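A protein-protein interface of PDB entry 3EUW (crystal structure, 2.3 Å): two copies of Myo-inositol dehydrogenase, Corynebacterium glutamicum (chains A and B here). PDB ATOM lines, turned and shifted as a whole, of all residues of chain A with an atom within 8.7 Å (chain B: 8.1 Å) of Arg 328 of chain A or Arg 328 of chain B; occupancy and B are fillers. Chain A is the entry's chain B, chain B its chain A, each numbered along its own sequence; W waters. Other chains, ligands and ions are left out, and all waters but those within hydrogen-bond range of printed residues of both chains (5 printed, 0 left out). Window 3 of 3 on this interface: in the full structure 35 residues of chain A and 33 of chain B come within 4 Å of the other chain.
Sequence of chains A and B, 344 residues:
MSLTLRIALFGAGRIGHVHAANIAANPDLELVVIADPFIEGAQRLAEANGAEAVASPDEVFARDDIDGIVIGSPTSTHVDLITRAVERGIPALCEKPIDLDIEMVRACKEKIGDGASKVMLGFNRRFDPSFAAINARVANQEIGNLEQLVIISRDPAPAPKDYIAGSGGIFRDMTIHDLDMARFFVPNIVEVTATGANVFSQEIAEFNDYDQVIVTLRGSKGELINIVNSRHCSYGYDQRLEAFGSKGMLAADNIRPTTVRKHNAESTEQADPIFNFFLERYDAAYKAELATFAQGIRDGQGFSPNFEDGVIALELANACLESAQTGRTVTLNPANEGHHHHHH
The backbone NH (N) of Thr 329 of chain B lies within hydrogen-bond range of the backbone carbonyl oxygen (O) of Gly 327 of chain A (2.8 Å). The backbone NH (N) of Thr 329 of chain A is in hydrogen-bond range of the backbone carbonyl oxygen (O) of Gly 327 of chain B, at 2.8 Å.
The side-chain hydroxyl (OG) of Ser 323 of chain A sits at hydrogen-bond distance from the backbone carbonyl oxygen (O) of Arg 328 of chain A (2.7 Å). OG1 of Thr 326 of chain A sits close to N of Arg 328 of chain A. The side-chain hydroxyl (OG1) of Thr 193 of chain A lies within hydrogen-bond range of the side-chain hydroxyl (OG1) of Thr 329 of chain A (2.6 Å). The side-chain hydroxyl (OG1) of Thr 329 of chain B lies within hydrogen-bond range of the side-chain hydroxyl (OG1) of Thr 193 of chain B (2.9 Å). The side-chain hydroxyl (OG) of Ser 323 of chain B sits at hydrogen-bond distance from the backbone carbonyl oxygen (O) of Arg 328 of chain B (2.7 Å).
Thr 193 of chain B touches Thr 193 of chain A (CG2 to CG2, 3.7 Å). O of Gly 327 of chain A touches CA of Arg 328 of chain B (3.5 Å). O of Gly 327 of chain B touches CA of Arg 328 of chain A (3.6 Å). Arg 328 of chain B touches Arg 328 of chain A.
Arg 328 of chain A touches two residues of chain B. Of chain A, only Gly 327 (3.5 Å) and Arg 328 (3.9 Å) come within 4 Å of Arg 328 of chain B. Gly 327 of chain A touches just these residues of chain B: Arg 328 and Thr 329. Of chain A, only Arg 328 (3.6 Å) and Thr 329 (2.8 Å) come within 4 Å of Gly 327 of chain B. Of the printed residues of chain A, Thr 193 of chain B touches Thr 193 (3.7 Å). Of the printed residues of chain A, Thr 329 of chain B touches Gly 327 (2.8 Å). The nearest residue of chain A that does not touch Arg 328 of chain B is Thr 329 of chain A (4.4 Å).
Along chain A the printed residues that touch a printed residue of chain B span positions 193 to 329. Among the printed residues, no Asp or Glu carboxylate lies within 4 Å of a Lys or Arg side-chain nitrogen of the other chain.
Thr 193 of chain B touches its own counterpart, Thr 193 of chain A. Gly 327 of chain A touches Arg 328 of chain B, and with the chains exchanged Arg 328 of chain A touches Gly 327 of chain B. Gly 327 of chain A touches Thr 329 of chain B, and with the chains exchanged Thr 329 of chain A touches Gly 327 of chain B. Arg 328 of chain B touches its own counterpart, Arg 328 of chain A. Of the 6 pairs that touch across the chains among the printed residues, 6 have their exchanged pair printed and touching as well.
Water W3 lies within hydrogen-bond range of OG1 of Thr 195 of chain A (2.6 Å), OG1 of Thr 329 of chain B (2.9 Å) and O of Ala 194 of chain A (3.5 Å). Water W2 lies within hydrogen-bond range of OG1 of Thr 329 of chain B (2.7 Å), O of Gly 327 of chain A (3.1 Å) and N of Arg 328 of chain A (3.3 Å). Water W1 lies within hydrogen-bond range of the side-chain hydroxyl of Thr 329 of chain A (2.7 Å), the backbone NH of Arg 328 of chain B (2.8 Å) and the backbone carbonyl oxygen of Gly 327 of chain B (3.1 Å). Water W4 lies within hydrogen-bond range of the backbone carbonyl oxygen (O) of Gly 327 of chain A, the guanidinium group (NH1) of Arg 328 of chain B and the backbone carbonyl oxygen (O) of Thr 329 of chain B. Water W5 lies within hydrogen-bond range of the side-chain hydroxyl of Thr 195 of chain B, the backbone carbonyl oxygen of Ala 194 of chain B and the side-chain hydroxyl of Thr 329 of chain A.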
ATOM      1  N   GLU A 191      27.614  23.987   2.797  1.00  0.00           N
ATOM      2  CA  GLU A 191      27.235  22.595   2.572  1.00  0.00           C
ATOM      3  C   GLU A 191      25.741  22.363   2.674  1.00  0.00           C
ATOM      4  O   GLU A 191      25.036  23.075   3.389  1.00  0.00           O
ATOM      5  CB  GLU A 191      27.940  21.658   3.553  1.00  0.00           C
ATOM      6  CG  GLU A 191      29.455  21.765   3.546  1.00  0.00           C
ATOM      7  CD  GLU A 191      30.119  20.589   4.240  1.00  0.00           C
ATOM      8  OE1 GLU A 191      29.667  20.204   5.341  1.00  0.00           O
ATOM      9  OE2 GLU A 191      31.096  20.047   3.686  1.00  0.00           O
ATOM     10  N   VAL A 192      25.276  21.342   1.968  1.00  0.00           N
ATOM     11  CA  VAL A 192      23.867  20.992   1.933  1.00  0.00           C
ATOM     12  C   VAL A 192      23.662  19.493   2.097  1.00  0.00           C
ATOM     13  O   VAL A 192      24.330  18.689   1.450  1.00  0.00           O
ATOM     14  CB  VAL A 192      23.220  21.411   0.589  1.00  0.00           C
ATOM     15  CG1 VAL A 192      21.742  20.967   0.553  1.00  0.00           C
ATOM     16  CG2 VAL A 192      23.346  22.930   0.394  1.00  0.00           C
ATOM     17  N   THR A 193      22.740  19.134   2.979  1.00  0.00           N
ATOM     18  CA  THR A 193      22.399  17.742   3.228  1.00  0.00           C
ATOM     19  C   THR A 193      20.874  17.707   3.325  1.00  0.00           C
ATOM     20  O   THR A 193      20.273  18.491   4.059  1.00  0.00           O
ATOM     21  CB  THR A 193      23.032  17.233   4.545  1.00  0.00           C
ATOM     22  OG1 THR A 193      24.455  17.405   4.493  1.00  0.00           O
ATOM     23  CG2 THR A 193      22.732  15.762   4.744  1.00  0.00           C
ATOM     24  N   ALA A 194      20.247  16.810   2.576  1.00  0.00           N
ATOM     25  CA  ALA A 194      18.798  16.720   2.567  1.00  0.00           C
ATOM     26  C   ALA A 194      18.348  15.275   2.549  1.00  0.00           C
ATOM     27  O   ALA A 194      19.054  14.403   2.043  1.00  0.00           O
ATOM     28  CB  ALA A 194      18.236  17.465   1.351  1.00  0.00           C
ATOM     29  N   THR A 195      17.164  15.036   3.103  1.00  0.00           N
ATOM     30  CA  THR A 195      16.601  13.699   3.182  1.00  0.00           C
ATOM     31  C   THR A 195      15.112  13.732   2.878  1.00  0.00           C
ATOM     32  O   THR A 195      14.358  14.481   3.509  1.00  0.00           O
ATOM     33  CB  THR A 195      16.810  13.120   4.584  1.00  0.00           C
ATOM     34  OG1 THR A 195      18.206  13.162   4.901  1.00  0.00           O
ATOM     35  CG2 THR A 195      16.308  11.690   4.659  1.00  0.00           C
ATOM     36  N   ALA A 319      20.766  21.519  -5.017  1.00  0.00           N
ATOM     37  CA  ALA A 319      21.750  20.816  -4.203  1.00  0.00           C
ATOM     38  C   ALA A 319      21.035  19.872  -3.248  1.00  0.00           C
ATOM     39  O   ALA A 319      21.493  18.754  -3.031  1.00  0.00           O
ATOM     40  CB  ALA A 319      22.618  21.814  -3.416  1.00  0.00           C
ATOM     41  N   CYS A 320      19.919  20.324  -2.678  1.00  0.00           N
ATOM     42  CA  CYS A 320      19.152  19.487  -1.761  1.00  0.00           C
ATOM     43  C   CYS A 320      18.713  18.214  -2.482  1.00  0.00           C
ATOM     44  O   CYS A 320      18.879  17.103  -1.964  1.00  0.00           O
ATOM     45  CB  CYS A 320      17.908  20.226  -1.245  1.00  0.00           C
ATOM     46  SG  CYS A 320      18.218  21.610  -0.113  1.00  0.00           S
ATOM     47  N   LEU A 321      18.155  18.384  -3.680  1.00  0.00           N
ATOM     48  CA  LEU A 321      17.678  17.256  -4.477  1.00  0.00           C
ATOM     49  C   LEU A 321      18.822  16.302  -4.772  1.00  0.00           C
ATOM     50  O   LEU A 321      18.676  15.086  -4.653  1.00  0.00           O
ATOM     51  CB  LEU A 321      17.055  17.742  -5.797  1.00  0.00           C
ATOM     52  CG  LEU A 321      16.380  16.679  -6.677  1.00  0.00           C
ATOM     53  CD1 LEU A 321      15.218  16.031  -5.919  1.00  0.00           C
ATOM     54  CD2 LEU A 321      15.884  17.328  -7.976  1.00  0.00           C
ATOM     55  N   GLU A 322      19.966  16.861  -5.154  1.00  0.00           N
ATOM     56  CA  GLU A 322      21.135  16.049  -5.454  1.00  0.00           C
ATOM     57  C   GLU A 322      21.592  15.299  -4.201  1.00  0.00           C
ATOM     58  O   GLU A 322      22.072  14.164  -4.281  1.00  0.00           O
ATOM     59  CB  GLU A 322      22.281  16.922  -5.956  1.00  0.00           C
ATOM     60  CG  GLU A 322      23.395  16.131  -6.600  1.00  0.00           C
ATOM     61  CD  GLU A 322      24.701  16.901  -6.672  1.00  0.00           C
ATOM     62  OE1 GLU A 322      24.667  18.132  -6.909  1.00  0.00           O
ATOM     63  OE2 GLU A 322      25.764  16.263  -6.501  1.00  0.00           O
ATOM     64  N   SER A 323      21.444  15.944  -3.046  1.00  0.00           N
ATOM     65  CA  SER A 323      21.854  15.337  -1.781  1.00  0.00           C
ATOM     66  C   SER A 323      20.932  14.185  -1.417  1.00  0.00           C
ATOM     67  O   SER A 323      21.390  13.122  -1.013  1.00  0.00           O
ATOM     68  CB  SER A 323      21.854  16.380  -0.655  1.00  0.00           C
ATOM     69  OG  SER A 323      22.177  15.767   0.580  1.00  0.00           O
ATOM     70  N   ALA A 324      19.636  14.405  -1.583  1.00  0.00           N
ATOM     71  CA  ALA A 324      18.637  13.392  -1.286  1.00  0.00           C
ATOM     72  C   ALA A 324      18.764  12.172  -2.203  1.00  0.00           C
ATOM     73  O   ALA A 324      18.655  11.033  -1.748  1.00  0.00           O
ATOM     74  CB  ALA A 324      17.249  13.987  -1.420  1.00  0.00           C
ATOM     75  N   GLN A 325      18.994  12.414  -3.490  1.00  0.00           N
ATOM     76  CA  GLN A 325      19.125  11.331  -4.461  1.00  0.00           C
ATOM     77  C   GLN A 325      20.363  10.477  -4.230  1.00  0.00           C
ATOM     78  O   GLN A 325      20.321   9.265  -4.422  1.00  0.00           O
ATOM     79  CB  GLN A 325      19.149  11.893  -5.895  1.00  0.00           C
ATOM     80  CG  GLN A 325      17.916  12.713  -6.231  1.00  0.00           C
ATOM     81  CD  GLN A 325      17.902  13.248  -7.649  1.00  0.00           C
ATOM     82  OE1 GLN A 325      18.902  13.778  -8.139  1.00  0.00           O
ATOM     83  NE2 GLN A 325      16.756  13.130  -8.313  1.00  0.00           N
ATOM     84  N   THR A 326      21.456  11.105  -3.801  1.00  0.00           N
ATOM     85  CA  THR A 326      22.706  10.389  -3.577  1.00  0.00           C
ATOM     86  C   THR A 326      22.960   9.982  -2.123  1.00  0.00           C
ATOM     87  O   THR A 326      23.868   9.195  -1.844  1.00  0.00           O
ATOM     88  CB  THR A 326      23.913  11.221  -4.070  1.00  0.00           C
ATOM     89  OG1 THR A 326      24.057  12.392  -3.259  1.00  0.00           O
ATOM     90  CG2 THR A 326      23.714  11.648  -5.524  1.00  0.00           C
ATOM     91  N   GLY A 327      22.169  10.513  -1.195  1.00  0.00           N
ATOM     92  CA  GLY A 327      22.371  10.169   0.203  1.00  0.00           C
ATOM     93  C   GLY A 327      23.739  10.652   0.660  1.00  0.00           C
ATOM     94  O   GLY A 327      24.389  10.038   1.501  1.00  0.00           O
ATOM     95  N   ARG A 328      24.171  11.773   0.097  1.00  0.00           N
ATOM     96  CA  ARG A 328      25.459  12.345   0.433  1.00  0.00           C
ATOM     97  C   ARG A 328      25.330  13.856   0.558  1.00  0.00           C
ATOM     98  O   ARG A 328      24.470  14.461  -0.067  1.00  0.00           O
ATOM     99  CB  ARG A 328      26.487  12.013  -0.667  1.00  0.00           C
ATOM    100  CG  ARG A 328      26.774  10.525  -0.846  1.00  0.00           C
ATOM    101  CD  ARG A 328      27.463  10.246  -2.179  1.00  0.00           C
ATOM    102  NE  ARG A 328      28.777  10.874  -2.288  1.00  0.00           N
ATOM    103  CZ  ARG A 328      29.853  10.474  -1.618  1.00  0.00           C
ATOM    104  NH1 ARG A 328      29.773   9.443  -0.782  1.00  0.00           N
ATOM    105  NH2 ARG A 328      31.011  11.093  -1.792  1.00  0.00           N
ATOM    106  N   THR A 329      26.190  14.441   1.386  1.00  0.00           N
ATOM    107  CA  THR A 329      26.244  15.875   1.601  1.00  0.00           C
ATOM    108  C   THR A 329      26.890  16.505   0.356  1.00  0.00           C
ATOM    109  O   THR A 329      27.810  15.930  -0.222  1.00  0.00           O
ATOM    110  CB  THR A 329      27.114  16.185   2.849  1.00  0.00           C
ATOM    111  OG1 THR A 329      26.416  15.777   4.027  1.00  0.00           O
ATOM    112  CG2 THR A 329      27.459  17.666   2.935  1.00  0.00           C
ATOM    113  N   VAL A 330      26.408  17.673  -0.055  1.00  0.00           N
ATOM    114  CA  VAL A 330      26.949  18.374  -1.226  1.00  0.00           C
ATOM    115  C   VAL A 330      27.732  19.634  -0.839  1.00  0.00           C
ATOM    116  O   VAL A 330      27.241  20.476  -0.076  1.00  0.00           O
ATOM    117  CB  VAL A 330      25.807  18.810  -2.191  1.00  0.00           C
ATOM    118  CG1 VAL A 330      26.344  19.774  -3.255  1.00  0.00           C
ATOM    119  CG2 VAL A 330      25.185  17.594  -2.849  1.00  0.00           C
ATOM    120  N   THR A 331      28.945  19.767  -1.367  1.00  0.00           N
ATOM    121  CA  THR A 331      29.765  20.945  -1.098  1.00  0.00           C
ATOM    122  C   THR A 331      29.370  21.967  -2.166  1.00  0.00           C
ATOM    123  O   THR A 331      29.552  21.731  -3.356  1.00  0.00           O
ATOM    124  CB  THR A 331      31.270  20.629  -1.207  1.00  0.00           C
ATOM    125  OG1 THR A 331      31.600  19.527  -0.350  1.00  0.00           O
ATOM    126  CG2 THR A 331      32.088  21.824  -0.781  1.00  0.00           C
ATOM    127  N   VAL B 192      20.927   6.471   8.745  1.00  0.00           N
ATOM    128  CA  VAL B 192      21.372   7.491   9.670  1.00  0.00           C
ATOM    129  C   VAL B 192      22.181   8.590   8.994  1.00  0.00           C
ATOM    130  O   VAL B 192      23.137   8.319   8.273  1.00  0.00           O
ATOM    131  CB  VAL B 192      22.228   6.868  10.784  1.00  0.00           C
ATOM    132  CG1 VAL B 192      22.814   7.950  11.668  1.00  0.00           C
ATOM    133  CG2 VAL B 192      21.371   5.919  11.614  1.00  0.00           C
ATOM    134  N   THR B 193      21.780   9.834   9.234  1.00  0.00           N
ATOM    135  CA  THR B 193      22.476  10.986   8.672  1.00  0.00           C
ATOM    136  C   THR B 193      22.786  11.953   9.811  1.00  0.00           C
ATOM    137  O   THR B 193      21.918  12.250  10.626  1.00  0.00           O
ATOM    138  CB  THR B 193      21.614  11.691   7.618  1.00  0.00           C
ATOM    139  OG1 THR B 193      21.144  10.722   6.678  1.00  0.00           O
ATOM    140  CG2 THR B 193      22.425  12.725   6.863  1.00  0.00           C
ATOM    141  N   ALA B 194      24.019  12.438   9.877  1.00  0.00           N
ATOM    142  CA  ALA B 194      24.390  13.353  10.948  1.00  0.00           C
ATOM    143  C   ALA B 194      25.348  14.429  10.480  1.00  0.00           C
ATOM    144  O   ALA B 194      26.206  14.185   9.634  1.00  0.00           O
ATOM    145  CB  ALA B 194      25.014  12.575  12.123  1.00  0.00           C
ATOM    146  N   THR B 195      25.205  15.615  11.064  1.00  0.00           N
ATOM    147  CA  THR B 195      26.038  16.760  10.737  1.00  0.00           C
ATOM    148  C   THR B 195      26.560  17.380  12.036  1.00  0.00           C
ATOM    149  O   THR B 195      25.779  17.705  12.931  1.00  0.00           O
ATOM    150  CB  THR B 195      25.216  17.808   9.979  1.00  0.00           C
ATOM    151  OG1 THR B 195      24.581  17.185   8.859  1.00  0.00           O
ATOM    152  CG2 THR B 195      26.104  18.937   9.492  1.00  0.00           C
ATOM    153  N   ALA B 319      26.852   5.139  14.208  1.00  0.00           N
ATOM    154  CA  ALA B 319      26.487   5.429  12.831  1.00  0.00           C
ATOM    155  C   ALA B 319      26.459   6.939  12.631  1.00  0.00           C
ATOM    156  O   ALA B 319      26.865   7.432  11.571  1.00  0.00           O
ATOM    157  CB  ALA B 319      25.133   4.821  12.488  1.00  0.00           C
ATOM    158  N   CYS B 320      25.994   7.668  13.649  1.00  0.00           N
ATOM    159  CA  CYS B 320      25.929   9.131  13.587  1.00  0.00           C
ATOM    160  C   CYS B 320      27.316   9.724  13.410  1.00  0.00           C
ATOM    161  O   CYS B 320      27.536  10.532  12.511  1.00  0.00           O
ATOM    162  CB  CYS B 320      25.315   9.729  14.860  1.00  0.00           C
ATOM    163  SG  CYS B 320      23.527   9.591  15.016  1.00  0.00           S
ATOM    164  N   LEU B 321      28.243   9.327  14.279  1.00  0.00           N
ATOM    165  CA  LEU B 321      29.614   9.813  14.225  1.00  0.00           C
ATOM    166  C   LEU B 321      30.226   9.546  12.860  1.00  0.00           C
ATOM    167  O   LEU B 321      30.870  10.417  12.280  1.00  0.00           O
ATOM    168  CB  LEU B 321      30.475   9.136  15.303  1.00  0.00           C
ATOM    169  CG  LEU B 321      31.956   9.541  15.352  1.00  0.00           C
ATOM    170  CD1 LEU B 321      32.072  11.030  15.620  1.00  0.00           C
ATOM    171  CD2 LEU B 321      32.677   8.760  16.437  1.00  0.00           C
ATOM    172  N   GLU B 322      30.027   8.337  12.350  1.00  0.00           N
ATOM    173  CA  GLU B 322      30.579   7.974  11.048  1.00  0.00           C
ATOM    174  C   GLU B 322      29.986   8.835   9.930  1.00  0.00           C
ATOM    175  O   GLU B 322      30.702   9.264   9.025  1.00  0.00           O
ATOM    176  CB  GLU B 322      30.315   6.500  10.769  1.00  0.00           C
ATOM    177  CG  GLU B 322      31.504   5.769  10.178  1.00  0.00           C
ATOM    178  CD  GLU B 322      31.412   5.667   8.686  1.00  0.00           C
ATOM    179  OE1 GLU B 322      30.321   5.318   8.195  1.00  0.00           O
ATOM    180  OE2 GLU B 322      32.416   5.920   8.004  1.00  0.00           O
ATOM    181  N   SER B 323      28.676   9.074   9.990  1.00  0.00           N
ATOM    182  CA  SER B 323      28.010   9.901   8.987  1.00  0.00           C
ATOM    183  C   SER B 323      28.560  11.325   9.065  1.00  0.00           C
ATOM    184  O   SER B 323      28.895  11.931   8.053  1.00  0.00           O
ATOM    185  CB  SER B 323      26.496   9.928   9.228  1.00  0.00           C
ATOM    186  OG  SER B 323      25.851  10.812   8.324  1.00  0.00           O
ATOM    187  N   ALA B 324      28.663  11.849  10.279  1.00  0.00           N
ATOM    188  CA  ALA B 324      29.158  13.208  10.472  1.00  0.00           C
ATOM    189  C   ALA B 324      30.580  13.360   9.961  1.00  0.00           C
ATOM    190  O   ALA B 324      30.940  14.394   9.409  1.00  0.00           O
ATOM    191  CB  ALA B 324      29.102  13.582  11.932  1.00  0.00           C
ATOM    192  N   GLN B 325      31.391  12.326  10.144  1.00  0.00           N
ATOM    193  CA  GLN B 325      32.776  12.375   9.694  1.00  0.00           C
ATOM    194  C   GLN B 325      32.932  12.153   8.191  1.00  0.00           C
ATOM    195  O   GLN B 325      33.953  12.537   7.610  1.00  0.00           O
ATOM    196  CB  GLN B 325      33.611  11.326  10.430  1.00  0.00           C
ATOM    197  CG  GLN B 325      33.721  11.529  11.935  1.00  0.00           C
ATOM    198  CD  GLN B 325      34.512  10.420  12.622  1.00  0.00           C
ATOM    199  OE1 GLN B 325      34.259   9.234  12.402  1.00  0.00           O
ATOM    200  NE2 GLN B 325      35.465  10.804  13.461  1.00  0.00           N
ATOM    201  N   THR B 326      31.926  11.556   7.557  1.00  0.00           N
ATOM    202  CA  THR B 326      32.030  11.235   6.134  1.00  0.00           C
ATOM    203  C   THR B 326      31.195  12.038   5.155  1.00  0.00           C
ATOM    204  O   THR B 326      31.435  11.988   3.944  1.00  0.00           O
ATOM    205  CB  THR B 326      31.733   9.739   5.910  1.00  0.00           C
ATOM    206  OG1 THR B 326      30.423   9.431   6.410  1.00  0.00           O
ATOM    207  CG2 THR B 326      32.767   8.878   6.660  1.00  0.00           C
ATOM    208  N   GLY B 327      30.206  12.766   5.654  1.00  0.00           N
ATOM    209  CA  GLY B 327      29.384  13.558   4.761  1.00  0.00           C
ATOM    210  C   GLY B 327      28.428  12.729   3.927  1.00  0.00           C
ATOM    211  O   GLY B 327      28.129  13.077   2.787  1.00  0.00           O
ATOM    212  N   ARG B 328      27.953  11.617   4.484  1.00  0.00           N
ATOM    213  CA  ARG B 328      27.005  10.786   3.760  1.00  0.00           C
ATOM    214  C   ARG B 328      26.086  10.016   4.703  1.00  0.00           C
ATOM    215  O   ARG B 328      26.383   9.842   5.885  1.00  0.00           O
ATOM    216  CB  ARG B 328      27.737   9.799   2.852  1.00  0.00           C
ATOM    217  CG  ARG B 328      28.191   8.544   3.565  1.00  0.00           C
ATOM    218  CD  ARG B 328      28.960   7.610   2.648  1.00  0.00           C
ATOM    219  NE  ARG B 328      29.014   6.282   3.240  1.00  0.00           N
ATOM    220  CZ  ARG B 328      28.125   5.322   3.014  1.00  0.00           C
ATOM    221  NH1 ARG B 328      27.104   5.522   2.193  1.00  0.00           N
ATOM    222  NH2 ARG B 328      28.245   4.160   3.631  1.00  0.00           N
ATOM    223  N   THR B 329      24.967   9.556   4.166  1.00  0.00           N
ATOM    224  CA  THR B 329      24.016   8.794   4.947  1.00  0.00           C
ATOM    225  C   THR B 329      24.590   7.393   5.165  1.00  0.00           C
ATOM    226  O   THR B 329      25.313   6.870   4.310  1.00  0.00           O
ATOM    227  CB  THR B 329      22.660   8.725   4.218  1.00  0.00           C
ATOM    228  OG1 THR B 329      22.132  10.052   4.079  1.00  0.00           O
ATOM    229  CG2 THR B 329      21.670   7.877   4.989  1.00  0.00           C
ATOM    230  N   VAL B 330      24.289   6.802   6.317  1.00  0.00           N
ATOM    231  CA  VAL B 330      24.770   5.468   6.660  1.00  0.00           C
ATOM    232  C   VAL B 330      23.613   4.468   6.740  1.00  0.00           C
ATOM    233  O   VAL B 330      22.643   4.689   7.460  1.00  0.00           O
ATOM    234  CB  VAL B 330      25.524   5.477   8.031  1.00  0.00           C
ATOM    235  CG1 VAL B 330      25.863   4.049   8.469  1.00  0.00           C
ATOM    236  CG2 VAL B 330      26.800   6.293   7.925  1.00  0.00           C
ATOM    237  N   THR B 331      23.719   3.378   5.988  1.00  0.00           N
ATOM    238  CA  THR B 331      22.698   2.328   5.994  1.00  0.00           C
ATOM    239  C   THR B 331      23.076   1.300   7.058  1.00  0.00           C
ATOM    240  O   THR B 331      24.117   0.654   6.975  1.00  0.00           O
ATOM    241  CB  THR B 331      22.607   1.626   4.622  1.00  0.00           C
ATOM    242  OG1 THR B 331      22.157   2.561   3.635  1.00  0.00           O
ATOM    243  CG2 THR B 331      21.629   0.463   4.684  1.00  0.00           C
ATOM    244  N   LEU B 332      22.226   1.162   8.064  1.00  0.00           N
ATOM    245  CA  LEU B 332      22.466   0.241   9.166  1.00  0.00           C
ATOM    246  C   LEU B 332      22.581  -1.228   8.780  1.00  0.00           C
ATOM    247  O   LEU B 332      23.458  -1.934   9.274  1.00  0.00           O
ATOM    248  CB  LEU B 332      21.368   0.407  10.209  1.00  0.00           C
ATOM    249  CG  LEU B 332      21.358   1.783  10.870  1.00  0.00           C
ATOM    250  CD1 LEU B 332      20.122   1.934  11.733  1.00  0.00           C
ATOM    251  CD2 LEU B 332      22.620   1.944  11.696  1.00  0.00           C
HETATM  252  O   HOH W   1      25.626  13.241   4.536  1.00  0.00           O
HETATM  253  O   HOH W   2      23.301  12.293   3.268  1.00  0.00           O
HETATM  254  O   HOH W   3      19.591  11.358   3.583  1.00  0.00           O
HETATM  255  O   HOH W   4      24.967   7.273   1.262  1.00  0.00           O
HETATM  256  O   HOH W   5      27.113  16.422   7.331  1.00  0.00           O
